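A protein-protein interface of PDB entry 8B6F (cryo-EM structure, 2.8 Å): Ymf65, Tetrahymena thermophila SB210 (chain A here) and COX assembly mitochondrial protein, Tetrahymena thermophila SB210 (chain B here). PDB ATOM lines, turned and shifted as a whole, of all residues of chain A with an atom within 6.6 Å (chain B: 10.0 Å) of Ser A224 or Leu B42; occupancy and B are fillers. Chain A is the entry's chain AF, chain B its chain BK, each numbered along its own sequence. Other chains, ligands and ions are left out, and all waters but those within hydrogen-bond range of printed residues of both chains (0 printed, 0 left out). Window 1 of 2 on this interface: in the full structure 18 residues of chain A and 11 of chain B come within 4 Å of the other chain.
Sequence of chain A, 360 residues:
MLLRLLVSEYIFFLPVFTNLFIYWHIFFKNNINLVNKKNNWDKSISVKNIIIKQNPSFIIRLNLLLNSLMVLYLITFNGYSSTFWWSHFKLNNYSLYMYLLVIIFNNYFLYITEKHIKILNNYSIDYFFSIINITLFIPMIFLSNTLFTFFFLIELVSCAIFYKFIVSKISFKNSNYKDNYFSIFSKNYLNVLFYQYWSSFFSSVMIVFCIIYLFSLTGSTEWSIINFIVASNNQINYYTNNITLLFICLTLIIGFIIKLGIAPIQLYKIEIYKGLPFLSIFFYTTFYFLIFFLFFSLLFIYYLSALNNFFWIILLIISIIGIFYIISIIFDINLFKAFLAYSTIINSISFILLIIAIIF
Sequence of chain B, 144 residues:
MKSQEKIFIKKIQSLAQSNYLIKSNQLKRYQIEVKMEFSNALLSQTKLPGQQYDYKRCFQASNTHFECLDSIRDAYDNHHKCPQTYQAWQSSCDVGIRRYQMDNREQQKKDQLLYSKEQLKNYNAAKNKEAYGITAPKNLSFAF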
ATOM      1  N   LYS A  90      13.650 -23.341 -12.291  1.00  0.00           N
ATOM      2  CA  LYS A  90      14.126 -24.014 -13.489  1.00  0.00           C
ATOM      3  C   LYS A  90      14.741 -25.354 -13.117  1.00  0.00           C
ATOM      4  O   LYS A  90      15.449 -25.467 -12.113  1.00  0.00           O
ATOM      5  CB  LYS A  90      15.152 -23.153 -14.230  1.00  0.00           C
ATOM      6  CG  LYS A  90      15.804 -23.833 -15.435  1.00  0.00           C
ATOM      7  CD  LYS A  90      14.794 -24.222 -16.509  1.00  0.00           C
ATOM      8  CE  LYS A  90      14.290 -23.016 -17.281  1.00  0.00           C
ATOM      9  NZ  LYS A  90      15.363 -22.385 -18.097  1.00  0.00           N
ATOM     10  N   ASN A  92      16.959 -28.007 -15.007  1.00  0.00           N
ATOM     11  CA  ASN A  92      17.755 -28.425 -16.151  1.00  0.00           C
ATOM     12  C   ASN A  92      19.095 -28.954 -15.660  1.00  0.00           C
ATOM     13  O   ASN A  92      19.432 -28.859 -14.479  1.00  0.00           O
ATOM     14  CB  ASN A  92      17.951 -27.282 -17.157  1.00  0.00           C
ATOM     15  CG  ASN A  92      18.595 -26.061 -16.540  1.00  0.00           C
ATOM     16  OD1 ASN A  92      19.134 -26.119 -15.440  1.00  0.00           O
ATOM     17  ND2 ASN A  92      18.550 -24.947 -17.257  1.00  0.00           N
ATOM     18  N   ASN A 145      14.396 -19.404 -11.318  1.00  0.00           N
ATOM     19  CA  ASN A 145      14.066 -19.098 -12.701  1.00  0.00           C
ATOM     20  C   ASN A 145      13.714 -17.636 -12.922  1.00  0.00           C
ATOM     21  O   ASN A 145      13.582 -17.217 -14.076  1.00  0.00           O
ATOM     22  CB  ASN A 145      12.892 -19.966 -13.174  1.00  0.00           C
ATOM     23  CG  ASN A 145      12.651 -19.857 -14.662  1.00  0.00           C
ATOM     24  OD1 ASN A 145      13.576 -19.620 -15.436  1.00  0.00           O
ATOM     25  ND2 ASN A 145      11.400 -20.016 -15.072  1.00  0.00           N
ATOM     26  N   THR A 221       9.834 -10.978 -15.023  1.00  0.00           N
ATOM     27  CA  THR A 221      11.195 -10.935 -14.507  1.00  0.00           C
ATOM     28  C   THR A 221      11.909 -12.270 -14.689  1.00  0.00           C
ATOM     29  O   THR A 221      12.950 -12.494 -14.060  1.00  0.00           O
ATOM     30  CB  THR A 221      11.196 -10.516 -13.030  1.00  0.00           C
ATOM     31  OG1 THR A 221      12.534 -10.228 -12.607  1.00  0.00           O
ATOM     32  CG2 THR A 221      10.621 -11.602 -12.152  1.00  0.00           C
ATOM     33  N   GLU A 222      11.371 -13.160 -15.516  1.00  0.00           N
ATOM     34  CA  GLU A 222      12.028 -14.422 -15.814  1.00  0.00           C
ATOM     35  C   GLU A 222      13.271 -14.186 -16.664  1.00  0.00           C
ATOM     36  O   GLU A 222      13.312 -13.292 -17.511  1.00  0.00           O
ATOM     37  CB  GLU A 222      11.064 -15.355 -16.547  1.00  0.00           C
ATOM     38  CG  GLU A 222      11.644 -16.710 -16.893  1.00  0.00           C
ATOM     39  CD  GLU A 222      10.630 -17.605 -17.570  1.00  0.00           C
ATOM     40  OE1 GLU A 222       9.443 -17.219 -17.623  1.00  0.00           O
ATOM     41  OE2 GLU A 222      11.015 -18.690 -18.054  1.00  0.00           O
ATOM     42  N   TRP A 223      14.292 -15.013 -16.436  1.00  0.00           N
ATOM     43  CA  TRP A 223      15.562 -14.819 -17.125  1.00  0.00           C
ATOM     44  C   TRP A 223      15.396 -14.940 -18.633  1.00  0.00           C
ATOM     45  O   TRP A 223      15.871 -14.088 -19.391  1.00  0.00           O
ATOM     46  CB  TRP A 223      16.593 -15.833 -16.630  1.00  0.00           C
ATOM     47  CG  TRP A 223      16.818 -15.811 -15.159  1.00  0.00           C
ATOM     48  CD1 TRP A 223      16.646 -16.848 -14.293  1.00  0.00           C
ATOM     49  CD2 TRP A 223      17.261 -14.701 -14.374  1.00  0.00           C
ATOM     50  NE1 TRP A 223      16.956 -16.453 -13.016  1.00  0.00           N
ATOM     51  CE2 TRP A 223      17.338 -15.138 -13.039  1.00  0.00           C
ATOM     52  CE3 TRP A 223      17.604 -13.379 -14.672  1.00  0.00           C
ATOM     53  CZ2 TRP A 223      17.741 -14.304 -12.003  1.00  0.00           C
ATOM     54  CZ3 TRP A 223      18.004 -12.551 -13.642  1.00  0.00           C
ATOM     55  CH2 TRP A 223      18.070 -13.018 -12.323  1.00  0.00           C
ATOM     56  N   SER A 224      14.726 -15.999 -19.088  1.00  0.00           N
ATOM     57  CA  SER A 224      14.588 -16.218 -20.523  1.00  0.00           C
ATOM     58  C   SER A 224      13.813 -15.087 -21.183  1.00  0.00           C
ATOM     59  O   SER A 224      14.203 -14.596 -22.248  1.00  0.00           O
ATOM     60  CB  SER A 224      13.903 -17.558 -20.783  1.00  0.00           C
ATOM     61  OG  SER A 224      13.689 -17.753 -22.169  1.00  0.00           O
ATOM     62  N   ILE A 225      12.708 -14.663 -20.571  1.00  0.00           N
ATOM     63  CA  ILE A 225      11.911 -13.585 -21.144  1.00  0.00           C
ATOM     64  C   ILE A 225      12.700 -12.282 -21.153  1.00  0.00           C
ATOM     65  O   ILE A 225      12.636 -11.512 -22.116  1.00  0.00           O
ATOM     66  CB  ILE A 225      10.577 -13.439 -20.390  1.00  0.00           C
ATOM     67  CG1 ILE A 225       9.742 -14.718 -20.512  1.00  0.00           C
ATOM     68  CG2 ILE A 225       9.794 -12.243 -20.922  1.00  0.00           C
ATOM     69  CD1 ILE A 225       9.348 -15.088 -21.930  1.00  0.00           C
ATOM     70  N   ILE A 226      13.447 -12.005 -20.082  1.00  0.00           N
ATOM     71  CA  ILE A 226      14.245 -10.782 -20.038  1.00  0.00           C
ATOM     72  C   ILE A 226      15.251 -10.769 -21.180  1.00  0.00           C
ATOM     73  O   ILE A 226      15.366  -9.784 -21.917  1.00  0.00           O
ATOM     74  CB  ILE A 226      14.944 -10.646 -18.672  1.00  0.00           C
ATOM     75  CG1 ILE A 226      13.930 -10.280 -17.587  1.00  0.00           C
ATOM     76  CG2 ILE A 226      16.058  -9.596 -18.730  1.00  0.00           C
ATOM     77  CD1 ILE A 226      14.490 -10.357 -16.182  1.00  0.00           C
ATOM     78  N   ASN A 227      15.992 -11.863 -21.349  1.00  0.00           N
ATOM     79  CA  ASN A 227      16.995 -11.906 -22.407  1.00  0.00           C
ATOM     80  C   ASN A 227      16.349 -11.780 -23.779  1.00  0.00           C
ATOM     81  O   ASN A 227      16.837 -11.037 -24.638  1.00  0.00           O
ATOM     82  CB  ASN A 227      17.804 -13.197 -22.313  1.00  0.00           C
ATOM     83  CG  ASN A 227      18.676 -13.242 -21.083  1.00  0.00           C
ATOM     84  OD1 ASN A 227      19.783 -12.709 -21.074  1.00  0.00           O
ATOM     85  ND2 ASN A 227      18.184 -13.887 -20.036  1.00  0.00           N
ATOM     86  N   PHE A 228      15.251 -12.500 -24.006  1.00  0.00           N
ATOM     87  CA  PHE A 228      14.594 -12.444 -25.306  1.00  0.00           C
ATOM     88  C   PHE A 228      14.085 -11.041 -25.607  1.00  0.00           C
ATOM     89  O   PHE A 228      14.234 -10.545 -26.729  1.00  0.00           O
ATOM     90  CB  PHE A 228      13.447 -13.455 -25.346  1.00  0.00           C
ATOM     91  CG  PHE A 228      12.673 -13.441 -26.629  1.00  0.00           C
ATOM     92  CD1 PHE A 228      13.161 -14.074 -27.755  1.00  0.00           C
ATOM     93  CD2 PHE A 228      11.447 -12.803 -26.702  1.00  0.00           C
ATOM     94  CE1 PHE A 228      12.447 -14.064 -28.935  1.00  0.00           C
ATOM     95  CE2 PHE A 228      10.727 -12.791 -27.877  1.00  0.00           C
ATOM     96  CZ  PHE A 228      11.228 -13.423 -28.995  1.00  0.00           C
ATOM     97  N   ILE A 229      13.479 -10.384 -24.617  1.00  0.00           N
ATOM     98  CA  ILE A 229      12.949  -9.043 -24.835  1.00  0.00           C
ATOM     99  C   ILE A 229      14.073  -8.047 -25.094  1.00  0.00           C
ATOM    100  O   ILE A 229      13.953  -7.168 -25.954  1.00  0.00           O
ATOM    101  CB  ILE A 229      12.077  -8.614 -23.641  1.00  0.00           C
ATOM    102  CG1 ILE A 229      10.806  -9.466 -23.550  1.00  0.00           C
ATOM    103  CG2 ILE A 229      11.725  -7.141 -23.762  1.00  0.00           C
ATOM    104  CD1 ILE A 229       9.815  -9.260 -24.675  1.00  0.00           C
ATOM    105  N   TYR A 302      25.173 -15.950 -18.080  1.00  0.00           N
ATOM    106  CA  TYR A 302      24.039 -16.794 -18.437  1.00  0.00           C
ATOM    107  C   TYR A 302      22.693 -16.115 -18.254  1.00  0.00           C
ATOM    108  O   TYR A 302      21.861 -16.152 -19.168  1.00  0.00           O
ATOM    109  CB  TYR A 302      24.091 -18.082 -17.600  1.00  0.00           C
ATOM    110  CG  TYR A 302      22.876 -18.972 -17.719  1.00  0.00           C
ATOM    111  CD1 TYR A 302      22.502 -19.513 -18.942  1.00  0.00           C
ATOM    112  CD2 TYR A 302      22.133 -19.312 -16.599  1.00  0.00           C
ATOM    113  CE1 TYR A 302      21.404 -20.343 -19.050  1.00  0.00           C
ATOM    114  CE2 TYR A 302      21.034 -20.140 -16.696  1.00  0.00           C
ATOM    115  CZ  TYR A 302      20.675 -20.654 -17.922  1.00  0.00           C
ATOM    116  OH  TYR A 302      19.581 -21.481 -18.019  1.00  0.00           O
ATOM    117  N   TYR A 303      22.445 -15.495 -17.101  1.00  0.00           N
ATOM    118  CA  TYR A 303      21.100 -15.014 -16.804  1.00  0.00           C
ATOM    119  C   TYR A 303      20.798 -13.718 -17.549  1.00  0.00           C
ATOM    120  O   TYR A 303      19.872 -13.661 -18.364  1.00  0.00           O
ATOM    121  CB  TYR A 303      20.937 -14.828 -15.294  1.00  0.00           C
ATOM    122  CG  TYR A 303      21.019 -16.121 -14.511  1.00  0.00           C
ATOM    123  CD1 TYR A 303      19.991 -17.052 -14.561  1.00  0.00           C
ATOM    124  CD2 TYR A 303      22.123 -16.406 -13.716  1.00  0.00           C
ATOM    125  CE1 TYR A 303      20.060 -18.233 -13.847  1.00  0.00           C
ATOM    126  CE2 TYR A 303      22.201 -17.585 -12.997  1.00  0.00           C
ATOM    127  CZ  TYR A 303      21.168 -18.493 -13.069  1.00  0.00           C
ATOM    128  OH  TYR A 303      21.238 -19.667 -12.357  1.00  0.00           O
ATOM    129  N   MET B  36      21.284 -16.481 -23.520  1.00  0.00           N
ATOM    130  CA  MET B  36      20.213 -17.516 -23.539  1.00  0.00           C
ATOM    131  C   MET B  36      19.081 -17.090 -24.463  1.00  0.00           C
ATOM    132  O   MET B  36      18.163 -17.863 -24.730  1.00  0.00           O
ATOM    133  CB  MET B  36      19.681 -17.772 -22.128  1.00  0.00           C
ATOM    134  CG  MET B  36      19.108 -16.546 -21.445  1.00  0.00           C
ATOM    135  SD  MET B  36      18.714 -16.827 -19.709  1.00  0.00           S
ATOM    136  CE  MET B  36      17.562 -18.192 -19.827  1.00  0.00           C
ATOM    137  N   GLU B  37      19.146 -15.847 -24.943  1.00  0.00           N
ATOM    138  CA  GLU B  37      18.147 -15.376 -25.895  1.00  0.00           C
ATOM    139  C   GLU B  37      18.220 -16.152 -27.203  1.00  0.00           C
ATOM    140  O   GLU B  37      17.213 -16.271 -27.909  1.00  0.00           O
ATOM    141  CB  GLU B  37      18.325 -13.880 -26.157  1.00  0.00           C
ATOM    142  CG  GLU B  37      19.679 -13.481 -26.743  1.00  0.00           C
ATOM    143  CD  GLU B  37      20.746 -13.270 -25.688  1.00  0.00           C
ATOM    144  OE1 GLU B  37      20.535 -13.695 -24.535  1.00  0.00           O
ATOM    145  OE2 GLU B  37      21.795 -12.676 -26.011  1.00  0.00           O
ATOM    146  N   PHE B  38      19.394 -16.681 -27.542  1.00  0.00           N
ATOM    147  CA  PHE B  38      19.584 -17.448 -28.766  1.00  0.00           C
ATOM    148  C   PHE B  38      19.394 -18.943 -28.567  1.00  0.00           C
ATOM    149  O   PHE B  38      19.519 -19.701 -29.533  1.00  0.00           O
ATOM    150  CB  PHE B  38      20.989 -17.198 -29.326  1.00  0.00           C
ATOM    151  CG  PHE B  38      21.321 -15.749 -29.515  1.00  0.00           C
ATOM    152  CD1 PHE B  38      20.384 -14.870 -30.030  1.00  0.00           C
ATOM    153  CD2 PHE B  38      22.569 -15.265 -29.170  1.00  0.00           C
ATOM    154  CE1 PHE B  38      20.689 -13.536 -30.203  1.00  0.00           C
ATOM    155  CE2 PHE B  38      22.881 -13.932 -29.339  1.00  0.00           C
ATOM    156  CZ  PHE B  38      21.938 -13.065 -29.857  1.00  0.00           C
ATOM    157  N   SER B  39      19.093 -19.384 -27.350  1.00  0.00           N
ATOM    158  CA  SER B  39      19.046 -20.803 -27.022  1.00  0.00           C
ATOM    159  C   SER B  39      17.645 -21.340 -27.293  1.00  0.00           C
ATOM    160  O   SER B  39      16.692 -20.988 -26.594  1.00  0.00           O
ATOM    161  CB  SER B  39      19.450 -21.028 -25.569  1.00  0.00           C
ATOM    162  OG  SER B  39      19.395 -22.404 -25.245  1.00  0.00           O
ATOM    163  N   ASN B  40      17.523 -22.192 -28.313  1.00  0.00           N
ATOM    164  CA  ASN B  40      16.230 -22.791 -28.625  1.00  0.00           C
ATOM    165  C   ASN B  40      15.728 -23.652 -27.474  1.00  0.00           C
ATOM    166  O   ASN B  40      14.534 -23.641 -27.155  1.00  0.00           O
ATOM    167  CB  ASN B  40      16.328 -23.621 -29.904  1.00  0.00           C
ATOM    168  CG  ASN B  40      16.607 -22.774 -31.127  1.00  0.00           C
ATOM    169  OD1 ASN B  40      17.626 -22.943 -31.794  1.00  0.00           O
ATOM    170  ND2 ASN B  40      15.697 -21.856 -31.430  1.00  0.00           N
ATOM    171  N   ALA B  41      16.623 -24.415 -26.844  1.00  0.00           N
ATOM    172  CA  ALA B  41      16.214 -25.267 -25.733  1.00  0.00           C
ATOM    173  C   ALA B  41      15.678 -24.440 -24.572  1.00  0.00           C
ATOM    174  O   ALA B  41      14.614 -24.741 -24.021  1.00  0.00           O
ATOM    175  CB  ALA B  41      17.391 -26.129 -25.279  1.00  0.00           C
ATOM    176  N   LEU B  42      16.396 -23.384 -24.190  1.00  0.00           N
ATOM    177  CA  LEU B  42      15.951 -22.559 -23.072  1.00  0.00           C
ATOM    178  C   LEU B  42      14.659 -21.823 -23.404  1.00  0.00           C
ATOM    179  O   LEU B  42      13.810 -21.627 -22.528  1.00  0.00           O
ATOM    180  CB  LEU B  42      17.051 -21.577 -22.676  1.00  0.00           C
ATOM    181  CG  LEU B  42      18.352 -22.217 -22.184  1.00  0.00           C
ATOM    182  CD1 LEU B  42      19.426 -21.168 -21.975  1.00  0.00           C
ATOM    183  CD2 LEU B  42      18.124 -22.985 -20.897  1.00  0.00           C
ATOM    184  N   LEU B  43      14.491 -21.406 -24.659  1.00  0.00           N
ATOM    185  CA  LEU B  43      13.248 -20.752 -25.051  1.00  0.00           C
ATOM    186  C   LEU B  43      12.082 -21.731 -25.079  1.00  0.00           C
ATOM    187  O   LEU B  43      10.947 -21.347 -24.776  1.00  0.00           O
ATOM    188  CB  LEU B  43      13.412 -20.077 -26.412  1.00  0.00           C
ATOM    189  CG  LEU B  43      14.307 -18.834 -26.428  1.00  0.00           C
ATOM    190  CD1 LEU B  43      14.565 -18.382 -27.850  1.00  0.00           C
ATOM    191  CD2 LEU B  43      13.688 -17.704 -25.620  1.00  0.00           C
ATOM    192  N   SER B  44      12.332 -22.989 -25.444  1.00  0.00           N
ATOM    193  CA  SER B  44      11.262 -23.980 -25.425  1.00  0.00           C
ATOM    194  C   SER B  44      10.908 -24.389 -24.002  1.00  0.00           C
ATOM    195  O   SER B  44       9.773 -24.805 -23.742  1.00  0.00           O
ATOM    196  CB  SER B  44      11.662 -25.205 -26.248  1.00  0.00           C
ATOM    197  OG  SER B  44      12.810 -25.833 -25.705  1.00  0.00           O
ATOM    198  N   GLN B  45      11.861 -24.294 -23.074  1.00  0.00           N
ATOM    199  CA  GLN B  45      11.565 -24.561 -21.673  1.00  0.00           C
ATOM    200  C   GLN B  45      10.611 -23.534 -21.079  1.00  0.00           C
ATOM    201  O   GLN B  45       9.995 -23.806 -20.044  1.00  0.00           O
ATOM    202  CB  GLN B  45      12.862 -24.601 -20.867  1.00  0.00           C
ATOM    203  CG  GLN B  45      13.709 -25.829 -21.150  1.00  0.00           C
ATOM    204  CD  GLN B  45      15.070 -25.761 -20.492  1.00  0.00           C
ATOM    205  OE1 GLN B  45      15.307 -24.934 -19.614  1.00  0.00           O
ATOM    206  NE2 GLN B  45      15.978 -26.631 -20.920  1.00  0.00           N
ATOM    207  N   THR B  46      10.474 -22.367 -21.703  1.00  0.00           N
ATOM    208  CA  THR B  46       9.512 -21.379 -21.242  1.00  0.00           C
ATOM    209  C   THR B  46       8.091 -21.831 -21.567  1.00  0.00           C
ATOM    210  O   THR B  46       7.857 -22.640 -22.467  1.00  0.00           O
ATOM    211  CB  THR B  46       9.783 -20.016 -21.882  1.00  0.00           C
ATOM    212  OG1 THR B  46       9.736 -20.134 -23.309  1.00  0.00           O
ATOM    213  CG2 THR B  46      11.144 -19.486 -21.462  1.00  0.00           C
ATOM    214  N   LYS B  47       7.133 -21.293 -20.817  1.00  0.00           N
ATOM    215  CA  LYS B  47       5.744 -21.696 -20.972  1.00  0.00           C
ATOM    216  C   LYS B  47       4.847 -20.653 -20.324  1.00  0.00           C
ATOM    217  O   LYS B  47       5.298 -19.831 -19.522  1.00  0.00           O
ATOM    218  CB  LYS B  47       5.496 -23.077 -20.356  1.00  0.00           C
ATOM    219  CG  LYS B  47       5.966 -23.188 -18.911  1.00  0.00           C
ATOM    220  CD  LYS B  47       5.892 -24.617 -18.398  1.00  0.00           C
ATOM    221  CE  LYS B  47       4.462 -25.080 -18.212  1.00  0.00           C
ATOM    222  NZ  LYS B  47       3.735 -24.269 -17.196  1.00  0.00           N
ATOM    223  N   TYR B  53       1.880 -29.967 -20.846  1.00  0.00           N
ATOM    224  CA  TYR B  53       2.120 -30.824 -21.999  1.00  0.00           C
ATOM    225  C   TYR B  53       1.625 -32.231 -21.707  1.00  0.00           C
ATOM    226  O   TYR B  53       1.960 -32.806 -20.666  1.00  0.00           O
ATOM    227  CB  TYR B  53       3.610 -30.857 -22.356  1.00  0.00           C
ATOM    228  CG  TYR B  53       4.217 -29.490 -22.558  1.00  0.00           C
ATOM    229  CD1 TYR B  53       3.979 -28.768 -23.719  1.00  0.00           C
ATOM    230  CD2 TYR B  53       5.029 -28.922 -21.587  1.00  0.00           C
ATOM    231  CE1 TYR B  53       4.533 -27.517 -23.907  1.00  0.00           C
ATOM    232  CE2 TYR B  53       5.587 -27.671 -21.766  1.00  0.00           C
ATOM    233  CZ  TYR B  53       5.334 -26.975 -22.929  1.00  0.00           C
ATOM    234  OH  TYR B  53       5.888 -25.731 -23.113  1.00  0.00           O
ATOM    235  N   GLY B  96       7.656 -26.092 -29.441  1.00  0.00           N
ATOM    236  CA  GLY B  96       9.012 -26.361 -28.990  1.00  0.00           C
ATOM    237  C   GLY B  96       9.373 -27.829 -29.094  1.00  0.00           C
ATOM    238  O   GLY B  96      10.479 -28.178 -29.513  1.00  0.00           O
ATOM    239  N   TYR B 100      12.410 -29.405 -31.437  1.00  0.00           N
ATOM    240  CA  TYR B 100      13.435 -30.316 -30.943  1.00  0.00           C
ATOM    241  C   TYR B 100      13.412 -31.632 -31.709  1.00  0.00           C
ATOM    242  O   TYR B 100      14.465 -32.171 -32.067  1.00  0.00           O
ATOM    243  CB  TYR B 100      13.237 -30.566 -29.451  1.00  0.00           C
ATOM    244  CG  TYR B 100      14.173 -31.604 -28.882  1.00  0.00           C
ATOM    245  CD1 TYR B 100      15.424 -31.248 -28.403  1.00  0.00           C
ATOM    246  CD2 TYR B 100      13.802 -32.940 -28.820  1.00  0.00           C
ATOM    247  CE1 TYR B 100      16.282 -32.193 -27.882  1.00  0.00           C
ATOM    248  CE2 TYR B 100      14.653 -33.893 -28.302  1.00  0.00           C
ATOM    249  CZ  TYR B 100      15.891 -33.513 -27.833  1.00  0.00           C
ATOM    250  OH  TYR B 100      16.743 -34.458 -27.315  1.00  0.00           O
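The side-chain amide nitrogen (ND2) of Asn A145 is in hydrogen-bond range of the side-chain carboxylate (OE2) of Glu A222. The backbone NH (N) of Trp A223 sits close to the backbone carbonyl oxygen (O) of Asn A145, at 3.3 Å. The side-chain amide nitrogen (ND2) of Asn A227 sits at hydrogen-bond distance from the backbone carbonyl oxygen (O) of Trp A223 (2.4 Å). OD1 of Asn A227 lies close to O of Tyr A303, 2.9 Å away. The side-chain hydroxyl (OG) of Ser B39 sits close to the backbone NH (N) of Leu B42 (3.3 Å).
Lys A90 touches Leu B42 (NZ to CD2, 3.98 Å). Glu A222 touches Thr B46 (OE2 to CG2, 3.5 Å). Trp A223 touches Met B36. Met B36 touches Ser A224. Ser A224 touches Leu B42 (OG to O, 3.9 Å). CD2 of Leu B43 touches OG of Ser A224, 3.5 Å away. Ser A224 touches Thr B46 (OG to CG2, 3.2 Å). O of Asn A227 touches CB of Glu B37 (3.6 Å). Phe A228 touches Glu B37. OH of Tyr A302 touches CD2 of Leu B42, 3.6 Å away.
OE1 of Gln B45 is in hydrogen-bond range of NZ of Lys A90, 3.0 Å away. The side-chain amide nitrogen (ND2) of Asn A227 lies within hydrogen-bond range of the side-chain sulfur (SD) of Met B36 (3.0 Å). O of Tyr A302 sits close to SD of Met B36. O of Tyr A303 lies close to SD of Met B36 (3.6 Å).
Hydrophobic or aromatic side chains of chain A within 4 Å of the printed part of chain B: Trp A223 and Tyr A302. Among the printed residues, 14 pairs touch across the chains. Among the printed residues, no Asp or Glu carboxylate lies within 4 Å of a Lys or Arg side-chain nitrogen of the other chain.
Ser A224 touches just these residues of chain B: Met B36 (3.6 Å), Leu B42 (3.9 Å), Leu B43 (3.5 Å) and Thr B46 (3.2 Å). Leu B42 touches just these residues of chain A: Lys A90 (3.98 Å), Ser A224 (3.9 Å) and Tyr A302 (3.6 Å). Glu A222 touches one residue of chain B. No residue of chain B comes within 4 Å of Ile A225. Printed residues of chain A within 4 Å of Gln B45: Lys A90 (3.0 Å). Of the printed residues of chain B, Phe A228 touches Glu B37. Of the printed residues of chain A, Met B36 touches Trp A223, Ser A224, Asn A227, Tyr A302 and Tyr A303. Of the printed residues of chain A, Glu B37 touches Asn A227 and Phe A228. The nearest printed residue of chain A that does not touch Leu B43 is Phe A228 (4.2 Å).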
